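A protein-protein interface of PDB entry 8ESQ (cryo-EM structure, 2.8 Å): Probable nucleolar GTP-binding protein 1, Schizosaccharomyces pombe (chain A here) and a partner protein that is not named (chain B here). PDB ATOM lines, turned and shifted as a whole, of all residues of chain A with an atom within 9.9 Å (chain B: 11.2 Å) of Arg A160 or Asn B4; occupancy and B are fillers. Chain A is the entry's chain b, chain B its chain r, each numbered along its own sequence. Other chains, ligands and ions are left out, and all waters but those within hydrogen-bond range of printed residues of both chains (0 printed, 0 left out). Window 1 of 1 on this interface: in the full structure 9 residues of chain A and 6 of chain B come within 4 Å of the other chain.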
ATOM      1  N   ALA A   4      -1.578 -24.923 -17.619  1.00  0.00           N
ATOM      2  CA  ALA A   4      -0.139 -25.144 -17.709  1.00  0.00           C
ATOM      3  C   ALA A   4       0.484 -24.235 -18.762  1.00  0.00           C
ATOM      4  O   ALA A   4       1.393 -23.460 -18.467  1.00  0.00           O
ATOM      5  CB  ALA A   4       0.154 -26.602 -18.025  1.00  0.00           C
ATOM      6  N   VAL A   5      -0.013 -24.342 -19.997  1.00  0.00           N
ATOM      7  CA  VAL A   5       0.489 -23.502 -21.077  1.00  0.00           C
ATOM      8  C   VAL A   5       0.035 -22.057 -20.928  1.00  0.00           C
ATOM      9  O   VAL A   5       0.584 -21.169 -21.588  1.00  0.00           O
ATOM     10  CB  VAL A   5       0.051 -24.065 -22.442  1.00  0.00           C
ATOM     11  N   PHE A   6      -0.961 -21.797 -20.077  1.00  0.00           N
ATOM     12  CA  PHE A   6      -1.454 -20.437 -19.893  1.00  0.00           C
ATOM     13  C   PHE A   6      -0.411 -19.519 -19.270  1.00  0.00           C
ATOM     14  O   PHE A   6      -0.531 -18.295 -19.392  1.00  0.00           O
ATOM     15  CB  PHE A   6      -2.717 -20.449 -19.029  1.00  0.00           C
ATOM     16  N   LYS A   7       0.603 -20.080 -18.607  1.00  0.00           N
ATOM     17  CA  LYS A   7       1.683 -19.319 -17.973  1.00  0.00           C
ATOM     18  C   LYS A   7       1.060 -18.391 -16.937  1.00  0.00           C
ATOM     19  O   LYS A   7       0.416 -18.895 -16.001  1.00  0.00           O
ATOM     20  CB  LYS A   7       2.521 -18.641 -19.059  1.00  0.00           C
ATOM     21  N   ASN A   8       1.228 -17.072 -17.039  1.00  0.00           N
ATOM     22  CA  ASN A   8       0.697 -16.062 -16.128  1.00  0.00           C
ATOM     23  C   ASN A   8       1.279 -16.164 -14.725  1.00  0.00           C
ATOM     24  O   ASN A   8       0.869 -15.399 -13.844  1.00  0.00           O
ATOM     25  CB  ASN A   8      -0.836 -16.101 -16.035  1.00  0.00           C
ATOM     26  N   ILE A   9       2.215 -17.076 -14.482  1.00  0.00           N
ATOM     27  CA  ILE A   9       2.841 -17.205 -13.172  1.00  0.00           C
ATOM     28  C   ILE A   9       3.847 -16.077 -12.994  1.00  0.00           C
ATOM     29  O   ILE A   9       4.673 -15.820 -13.877  1.00  0.00           O
ATOM     30  CB  ILE A   9       3.511 -18.579 -13.021  1.00  0.00           C
ATOM     31  N   LEU A  82       2.603 -34.524 -21.108  1.00  0.00           N
ATOM     32  CA  LEU A  82       3.710 -33.702 -21.584  1.00  0.00           C
ATOM     33  C   LEU A  82       4.496 -33.109 -20.422  1.00  0.00           C
ATOM     34  O   LEU A  82       5.732 -33.074 -20.450  1.00  0.00           O
ATOM     35  CB  LEU A  82       3.187 -32.596 -22.499  1.00  0.00           C
ATOM     36  N   LEU A  86       8.404 -34.006 -19.670  1.00  0.00           N
ATOM     37  CA  LEU A  86       9.363 -32.921 -19.834  1.00  0.00           C
ATOM     38  C   LEU A  86       9.892 -32.370 -18.518  1.00  0.00           C
ATOM     39  O   LEU A  86      11.006 -31.833 -18.488  1.00  0.00           O
ATOM     40  CB  LEU A  86       8.732 -31.779 -20.637  1.00  0.00           C
ATOM     41  N   GLU A 152      11.207 -22.110 -10.654  1.00  0.00           N
ATOM     42  CA  GLU A 152      11.496 -21.085 -11.654  1.00  0.00           C
ATOM     43  C   GLU A 152      11.761 -21.708 -13.019  1.00  0.00           C
ATOM     44  O   GLU A 152      11.279 -21.213 -14.045  1.00  0.00           O
ATOM     45  CB  GLU A 152      12.687 -20.238 -11.206  1.00  0.00           C
ATOM     46  N   GLN A 153      12.534 -22.796 -13.051  1.00  0.00           N
ATOM     47  CA  GLN A 153      12.783 -23.488 -14.312  1.00  0.00           C
ATOM     48  C   GLN A 153      11.497 -24.076 -14.879  1.00  0.00           C
ATOM     49  O   GLN A 153      11.265 -24.027 -16.092  1.00  0.00           O
ATOM     50  CB  GLN A 153      13.833 -24.581 -14.113  1.00  0.00           C
ATOM     51  N   VAL A 154      10.653 -24.642 -14.014  1.00  0.00           N
ATOM     52  CA  VAL A 154       9.380 -25.196 -14.467  1.00  0.00           C
ATOM     53  C   VAL A 154       8.489 -24.096 -15.030  1.00  0.00           C
ATOM     54  O   VAL A 154       7.830 -24.277 -16.061  1.00  0.00           O
ATOM     55  CB  VAL A 154       8.688 -25.953 -13.320  1.00  0.00           C
ATOM     56  N   ARG A 155       8.449 -22.943 -14.357  1.00  0.00           N
ATOM     57  CA  ARG A 155       7.619 -21.838 -14.828  1.00  0.00           C
ATOM     58  C   ARG A 155       8.080 -21.341 -16.192  1.00  0.00           C
ATOM     59  O   ARG A 155       7.254 -21.057 -17.067  1.00  0.00           O
ATOM     60  CB  ARG A 155       7.635 -20.700 -13.809  1.00  0.00           C
ATOM     61  N   GLN A 156       9.394 -21.222 -16.389  1.00  0.00           N
ATOM     62  CA  GLN A 156       9.912 -20.777 -17.679  1.00  0.00           C
ATOM     63  C   GLN A 156       9.571 -21.773 -18.781  1.00  0.00           C
ATOM     64  O   GLN A 156       9.176 -21.384 -19.885  1.00  0.00           O
ATOM     65  CB  GLN A 156      11.424 -20.563 -17.591  1.00  0.00           C
ATOM     66  N   HIS A 157       9.723 -23.069 -18.497  1.00  0.00           N
ATOM     67  CA  HIS A 157       9.394 -24.087 -19.489  1.00  0.00           C
ATOM     68  C   HIS A 157       7.904 -24.090 -19.804  1.00  0.00           C
ATOM     69  O   HIS A 157       7.508 -24.213 -20.969  1.00  0.00           O
ATOM     70  CB  HIS A 157       9.843 -25.463 -19.000  1.00  0.00           C
ATOM     71  N   LEU A 158       7.061 -23.963 -18.776  1.00  0.00           N
ATOM     72  CA  LEU A 158       5.619 -23.942 -18.996  1.00  0.00           C
ATOM     73  C   LEU A 158       5.204 -22.727 -19.817  1.00  0.00           C
ATOM     74  O   LEU A 158       4.337 -22.827 -20.693  1.00  0.00           O
ATOM     75  CB  LEU A 158       4.882 -23.964 -17.658  1.00  0.00           C
ATOM     76  N   SER A 159       5.807 -21.568 -19.541  1.00  0.00           N
ATOM     77  CA  SER A 159       5.479 -20.366 -20.301  1.00  0.00           C
ATOM     78  C   SER A 159       5.859 -20.519 -21.768  1.00  0.00           C
ATOM     79  O   SER A 159       5.115 -20.094 -22.658  1.00  0.00           O
ATOM     80  CB  SER A 159       6.177 -19.152 -19.689  1.00  0.00           C
ATOM     81  N   ARG A 160       7.015 -21.126 -22.039  1.00  0.00           N
ATOM     82  CA  ARG A 160       7.460 -21.336 -23.409  1.00  0.00           C
ATOM     83  C   ARG A 160       6.757 -22.501 -24.093  1.00  0.00           C
ATOM     84  O   ARG A 160       6.931 -22.682 -25.303  1.00  0.00           O
ATOM     85  CB  ARG A 160       8.974 -21.560 -23.439  1.00  0.00           C
ATOM     86  N   LEU A 161       5.979 -23.291 -23.356  1.00  0.00           N
ATOM     87  CA  LEU A 161       5.305 -24.435 -23.946  1.00  0.00           C
ATOM     88  C   LEU A 161       4.215 -23.979 -24.916  1.00  0.00           C
ATOM     89  O   LEU A 161       3.600 -22.927 -24.724  1.00  0.00           O
ATOM     90  CB  LEU A 161       4.694 -25.315 -22.859  1.00  0.00           C
ATOM     91  N   PRO A 162       3.962 -24.754 -25.967  1.00  0.00           N
ATOM     92  CA  PRO A 162       2.906 -24.387 -26.917  1.00  0.00           C
ATOM     93  C   PRO A 162       1.523 -24.497 -26.294  1.00  0.00           C
ATOM     94  O   PRO A 162       1.274 -25.294 -25.388  1.00  0.00           O
ATOM     95  CB  PRO A 162       3.082 -25.401 -28.052  1.00  0.00           C
ATOM     96  N   ALA A 163       0.614 -23.669 -26.804  1.00  0.00           N
ATOM     97  CA  ALA A 163      -0.779 -23.677 -26.360  1.00  0.00           C
ATOM     98  C   ALA A 163      -1.619 -24.514 -27.323  1.00  0.00           C
ATOM     99  O   ALA A 163      -2.460 -24.015 -28.072  1.00  0.00           O
ATOM    100  CB  ALA A 163      -1.306 -22.251 -26.243  1.00  0.00           C
ATOM    101  N   ILE A 164      -1.369 -25.825 -27.290  1.00  0.00           N
ATOM    102  CA  ILE A 164      -2.088 -26.745 -28.161  1.00  0.00           C
ATOM    103  C   ILE A 164      -3.544 -26.845 -27.723  1.00  0.00           C
ATOM    104  O   ILE A 164      -3.881 -26.675 -26.543  1.00  0.00           O
ATOM    105  CB  ILE A 164      -1.414 -28.128 -28.166  1.00  0.00           C
ATOM    106  N   GLN A 192       6.894 -21.666 -38.693  1.00  0.00           N
ATOM    107  CA  GLN A 192       8.047 -22.144 -39.453  1.00  0.00           C
ATOM    108  C   GLN A 192       8.976 -22.863 -38.480  1.00  0.00           C
ATOM    109  O   GLN A 192       9.878 -22.255 -37.899  1.00  0.00           O
ATOM    110  CB  GLN A 192       8.756 -20.991 -40.164  1.00  0.00           C
ATOM    111  N   VAL A 193       8.750 -24.165 -38.305  1.00  0.00           N
ATOM    112  CA  VAL A 193       9.595 -24.959 -37.424  1.00  0.00           C
ATOM    113  C   VAL A 193      10.960 -25.142 -38.072  1.00  0.00           C
ATOM    114  O   VAL A 193      11.063 -25.518 -39.248  1.00  0.00           O
ATOM    115  CB  VAL A 193       8.936 -26.311 -37.117  1.00  0.00           C
ATOM    116  N   ASP A 194      12.016 -24.870 -37.309  1.00  0.00           N
ATOM    117  CA  ASP A 194      13.368 -24.980 -37.835  1.00  0.00           C
ATOM    118  C   ASP A 194      13.696 -26.427 -38.181  1.00  0.00           C
ATOM    119  O   ASP A 194      13.364 -27.353 -37.435  1.00  0.00           O
ATOM    120  CB  ASP A 194      14.377 -24.439 -36.822  1.00  0.00           C
ATOM    121  N   THR A 201      15.784 -32.661 -34.178  1.00  0.00           N
ATOM    122  CA  THR A 201      16.105 -31.252 -33.978  1.00  0.00           C
ATOM    123  C   THR A 201      14.962 -30.517 -33.290  1.00  0.00           C
ATOM    124  O   THR A 201      15.188 -29.713 -32.378  1.00  0.00           O
ATOM    125  CB  THR A 201      16.437 -30.591 -35.316  1.00  0.00           C
ATOM    126  N   THR A 202      13.724 -30.781 -33.712  1.00  0.00           N
ATOM    127  CA  THR A 202      12.544 -30.194 -33.078  1.00  0.00           C
ATOM    128  C   THR A 202      12.192 -31.043 -31.861  1.00  0.00           C
ATOM    129  O   THR A 202      11.307 -31.903 -31.889  1.00  0.00           O
ATOM    130  CB  THR A 202      11.385 -30.109 -34.062  1.00  0.00           C
ATOM    131  N   LYS A 203      12.914 -30.791 -30.766  1.00  0.00           N
ATOM    132  CA  LYS A 203      12.733 -31.585 -29.554  1.00  0.00           C
ATOM    133  C   LYS A 203      11.321 -31.445 -29.002  1.00  0.00           C
ATOM    134  O   LYS A 203      10.714 -32.433 -28.571  1.00  0.00           O
ATOM    135  CB  LYS A 203      13.763 -31.177 -28.502  1.00  0.00           C
ATOM    136  N   SER A 204      10.780 -30.233 -29.009  1.00  0.00           N
ATOM    137  CA  SER A 204       9.435 -29.977 -28.521  1.00  0.00           C
ATOM    138  C   SER A 204       8.465 -29.825 -29.686  1.00  0.00           C
ATOM    139  O   SER A 204       8.851 -29.515 -30.815  1.00  0.00           O
ATOM    140  CB  SER A 204       9.406 -28.723 -27.644  1.00  0.00           C
ATOM    141  N   LEU A 205       7.188 -30.054 -29.393  1.00  0.00           N
ATOM    142  CA  LEU A 205       6.158 -29.978 -30.416  1.00  0.00           C
ATOM    143  C   LEU A 205       5.948 -28.539 -30.875  1.00  0.00           C
ATOM    144  O   LEU A 205       6.090 -27.587 -30.102  1.00  0.00           O
ATOM    145  CB  LEU A 205       4.843 -30.554 -29.893  1.00  0.00           C
ATOM    146  N   PHE A 206       5.610 -28.390 -32.152  1.00  0.00           N
ATOM    147  CA  PHE A 206       5.285 -27.100 -32.743  1.00  0.00           C
ATOM    148  C   PHE A 206       3.899 -27.196 -33.362  1.00  0.00           C
ATOM    149  O   PHE A 206       3.645 -28.078 -34.189  1.00  0.00           O
ATOM    150  CB  PHE A 206       6.322 -26.693 -33.792  1.00  0.00           C
ATOM    151  N   VAL A 207       3.008 -26.292 -32.965  1.00  0.00           N
ATOM    152  CA  VAL A 207       1.618 -26.296 -33.405  1.00  0.00           C
ATOM    153  C   VAL A 207       1.407 -25.110 -34.332  1.00  0.00           C
ATOM    154  O   VAL A 207       1.837 -23.991 -34.026  1.00  0.00           O
ATOM    155  CB  VAL A 207       0.648 -26.244 -32.213  1.00  0.00           C
ATOM    156  N   ASP A 221       3.325 -30.598 -35.202  1.00  0.00           N
ATOM    157  CA  ASP A 221       4.487 -31.385 -35.577  1.00  0.00           C
ATOM    158  C   ASP A 221       5.107 -32.027 -34.342  1.00  0.00           C
ATOM    159  O   ASP A 221       5.088 -31.459 -33.248  1.00  0.00           O
ATOM    160  CB  ASP A 221       5.523 -30.516 -36.292  1.00  0.00           C
ATOM    161  N   PRO A 223       8.529 -34.611 -32.825  1.00  0.00           N
ATOM    162  CA  PRO A 223       9.891 -35.059 -33.127  1.00  0.00           C
ATOM    163  C   PRO A 223       9.902 -36.462 -33.714  1.00  0.00           C
ATOM    164  O   PRO A 223       9.041 -37.293 -33.415  1.00  0.00           O
ATOM    165  CB  PRO A 223      10.589 -35.019 -31.764  1.00  0.00           C
ATOM    166  N   GLN A 239       7.614 -37.502 -25.707  1.00  0.00           N
ATOM    167  CA  GLN A 239       6.637 -36.422 -25.787  1.00  0.00           C
ATOM    168  C   GLN A 239       5.744 -36.580 -27.011  1.00  0.00           C
ATOM    169  O   GLN A 239       4.537 -36.314 -26.947  1.00  0.00           O
ATOM    170  CB  GLN A 239       7.351 -35.070 -25.813  1.00  0.00           C
ATOM    171  N   PRO B   2       4.638 -17.758 -28.480  1.00  0.00           N
ATOM    172  CA  PRO B   2       5.371 -18.637 -29.396  1.00  0.00           C
ATOM    173  C   PRO B   2       5.737 -19.969 -28.750  1.00  0.00           C
ATOM    174  O   PRO B   2       5.211 -20.292 -27.686  1.00  0.00           O
ATOM    175  CB  PRO B   2       6.619 -17.824 -29.738  1.00  0.00           C
ATOM    176  CG  PRO B   2       6.217 -16.409 -29.519  1.00  0.00           C
ATOM    177  CD  PRO B   2       5.276 -16.437 -28.357  1.00  0.00           C
ATOM    178  N   GLN B   3       6.624 -20.733 -29.382  1.00  0.00           N
ATOM    179  CA  GLN B   3       6.974 -22.062 -28.905  1.00  0.00           C
ATOM    180  C   GLN B   3       8.428 -22.103 -28.460  1.00  0.00           C
ATOM    181  O   GLN B   3       9.323 -21.673 -29.193  1.00  0.00           O
ATOM    182  CB  GLN B   3       6.748 -23.127 -29.989  1.00  0.00           C
ATOM    183  CG  GLN B   3       5.305 -23.569 -30.157  1.00  0.00           C
ATOM    184  CD  GLN B   3       4.433 -22.501 -30.780  1.00  0.00           C
ATOM    185  OE1 GLN B   3       4.699 -22.029 -31.885  1.00  0.00           O
ATOM    186  NE2 GLN B   3       3.380 -22.114 -30.072  1.00  0.00           N
ATOM    187  N   ASN B   4       8.646 -22.630 -27.256  1.00  0.00           N
ATOM    188  CA  ASN B   4       9.970 -23.011 -26.745  1.00  0.00           C
ATOM    189  C   ASN B   4      10.907 -21.806 -26.828  1.00  0.00           C
ATOM    190  O   ASN B   4      10.588 -20.748 -26.268  1.00  0.00           O
ATOM    191  CB  ASN B   4      10.434 -24.250 -27.496  1.00  0.00           C
ATOM    192  CG  ASN B   4       9.310 -25.230 -27.749  1.00  0.00           C
ATOM    193  OD1 ASN B   4       9.018 -25.574 -28.894  1.00  0.00           O
ATOM    194  ND2 ASN B   4       8.662 -25.676 -26.680  1.00  0.00           N
ATOM    195  N   GLU B   5      12.058 -21.922 -27.488  1.00  0.00           N
ATOM    196  CA  GLU B   5      13.098 -20.894 -27.464  1.00  0.00           C
ATOM    197  C   GLU B   5      12.952 -19.989 -28.689  1.00  0.00           C
ATOM    198  O   GLU B   5      13.668 -20.108 -29.684  1.00  0.00           O
ATOM    199  CB  GLU B   5      14.471 -21.552 -27.422  1.00  0.00           C
ATOM    200  CG  GLU B   5      14.766 -22.300 -26.133  1.00  0.00           C
ATOM    201  CD  GLU B   5      16.246 -22.562 -25.944  1.00  0.00           C
ATOM    202  OE1 GLU B   5      16.948 -22.750 -26.959  1.00  0.00           O
ATOM    203  OE2 GLU B   5      16.708 -22.581 -24.783  1.00  0.00           O
ATOM    204  N   TYR B   6      11.999 -19.056 -28.600  1.00  0.00           N
ATOM    205  CA  TYR B   6      11.637 -18.300 -29.796  1.00  0.00           C
ATOM    206  C   TYR B   6      12.550 -17.097 -30.009  1.00  0.00           C
ATOM    207  O   TYR B   6      12.741 -16.657 -31.149  1.00  0.00           O
ATOM    208  CB  TYR B   6      10.166 -17.875 -29.756  1.00  0.00           C
ATOM    209  CG  TYR B   6       9.628 -17.392 -28.430  1.00  0.00           C
ATOM    210  CD1 TYR B   6       9.207 -18.288 -27.456  1.00  0.00           C
ATOM    211  CD2 TYR B   6       9.526 -16.034 -28.157  1.00  0.00           C
ATOM    212  CE1 TYR B   6       8.708 -17.847 -26.245  1.00  0.00           C
ATOM    213  CE2 TYR B   6       9.022 -15.583 -26.951  1.00  0.00           C
ATOM    214  CZ  TYR B   6       8.618 -16.495 -25.998  1.00  0.00           C
ATOM    215  OH  TYR B   6       8.119 -16.052 -24.795  1.00  0.00           O
ATOM    216  N   ILE B   7      13.121 -16.538 -28.939  1.00  0.00           N
ATOM    217  CA  ILE B   7      14.134 -15.506 -29.149  1.00  0.00           C
ATOM    218  C   ILE B   7      15.401 -16.128 -29.721  1.00  0.00           C
ATOM    219  O   ILE B   7      16.045 -15.550 -30.603  1.00  0.00           O
ATOM    220  CB  ILE B   7      14.412 -14.704 -27.860  1.00  0.00           C
ATOM    221  CG1 ILE B   7      15.056 -15.569 -26.778  1.00  0.00           C
ATOM    222  CG2 ILE B   7      13.146 -14.009 -27.366  1.00  0.00           C
ATOM    223  CD1 ILE B   7      15.497 -14.786 -25.557  1.00  0.00           C
ATOM    224  N   GLU B   8      15.756 -17.330 -29.256  1.00  0.00           N
ATOM    225  CA  GLU B   8      16.922 -18.019 -29.798  1.00  0.00           C
ATOM    226  C   GLU B   8      16.771 -18.260 -31.292  1.00  0.00           C
ATOM    227  O   GLU B   8      17.721 -18.065 -32.058  1.00  0.00           O
ATOM    228  CB  GLU B   8      17.142 -19.343 -29.068  1.00  0.00           C
ATOM    229  CG  GLU B   8      17.361 -19.209 -27.576  1.00  0.00           C
ATOM    230  CD  GLU B   8      18.614 -18.425 -27.245  1.00  0.00           C
ATOM    231  OE1 GLU B   8      19.595 -18.521 -28.012  1.00  0.00           O
ATOM    232  OE2 GLU B   8      18.621 -17.720 -26.215  1.00  0.00           O
ATOM    233  N   GLU B   9      15.581 -18.679 -31.726  1.00  0.00           N
ATOM    234  CA  GLU B   9      15.347 -18.869 -33.153  1.00  0.00           C
ATOM    235  C   GLU B   9      15.502 -17.559 -33.912  1.00  0.00           C
ATOM    236  O   GLU B   9      16.100 -17.527 -34.993  1.00  0.00           O
ATOM    237  CB  GLU B   9      13.960 -19.467 -33.381  1.00  0.00           C
ATOM    238  CG  GLU B   9      13.817 -20.883 -32.859  1.00  0.00           C
ATOM    239  CD  GLU B   9      12.429 -21.448 -33.077  1.00  0.00           C
ATOM    240  OE1 GLU B   9      11.530 -20.684 -33.486  1.00  0.00           O
ATOM    241  OE2 GLU B   9      12.239 -22.659 -32.836  1.00  0.00           O
ATOM    242  N   SER B  10      14.974 -16.466 -33.359  1.00  0.00           N
ATOM    243  CA  SER B  10      15.151 -15.166 -33.998  1.00  0.00           C
ATOM    244  C   SER B  10      16.603 -14.710 -33.925  1.00  0.00           C
ATOM    245  O   SER B  10      17.117 -14.108 -34.874  1.00  0.00           O
ATOM    246  CB  SER B  10      14.222 -14.131 -33.368  1.00  0.00           C
ATOM    247  OG  SER B  10      13.964 -14.432 -32.014  1.00  0.00           O
ATOM    248  N   ILE B  11      17.283 -14.981 -32.807  1.00  0.00           N
ATOM    249  CA  ILE B  11      18.720 -14.720 -32.749  1.00  0.00           C
ATOM    250  C   ILE B  11      19.448 -15.550 -33.796  1.00  0.00           C
ATOM    251  O   ILE B  11      20.357 -15.062 -34.477  1.00  0.00           O
ATOM    252  CB  ILE B  11      19.267 -14.985 -31.333  1.00  0.00           C
ATOM    253  CG1 ILE B  11      18.642 -14.021 -30.324  1.00  0.00           C
ATOM    254  CG2 ILE B  11      20.781 -14.861 -31.314  1.00  0.00           C
ATOM    255  CD1 ILE B  11      18.796 -14.462 -28.885  1.00  0.00           C
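The backbone carbonyl oxygen (O) of Arg A160 lies within hydrogen-bond range of the backbone NH (N) of Asn B4, at 2.6 Å.
O of Pro B2 touches O of Arg A160, at 3.8 Å. Gln B3 touches Arg A160. Gln B3 touches Pro A162 (CG to CB, 3.6 Å). ND2 of Asn B4 touches CB of Ser A204, at 3.3 Å. OD1 of Asn B4 touches O of Leu A205, 3.8 Å away.
Phe A6 touches none of the printed residues of chain B. No residue of chain B comes within 4 Å of His A157. No residue of chain B comes within 4 Å of Leu A158. No residue of chain B comes within 4 Å of Ser A159. Of chain B, only Pro B2, Gln B3 and Asn B4 come within 4 Å of Arg A160. No residue of chain B comes within 4 Å of Leu A161. Of chain B, only Gln B3 (3.6 Å) comes within 4 Å of Pro A162. Printed residues of chain A within 4 Å of Pro B2: Arg A160. Of the printed residues of chain A, Gln B3 touches Arg A160 and Pro A162. The nearest residue of chain B that does not touch Arg A160 is Tyr B6 (4.7 Å). The nearest residue of chain A that does not touch Asn B4 is Leu A161 (4.5 Å). The nearest printed residue of chain A that does not touch Gln B3 is Val A207 (4.1 Å).
Of the 34 printed residues of chain A, 4 touch a printed residue of chain B. Among the printed residues, no Asp or Glu carboxylate lies within 4 Å of a Lys or Arg side-chain nitrogen of the other chain.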
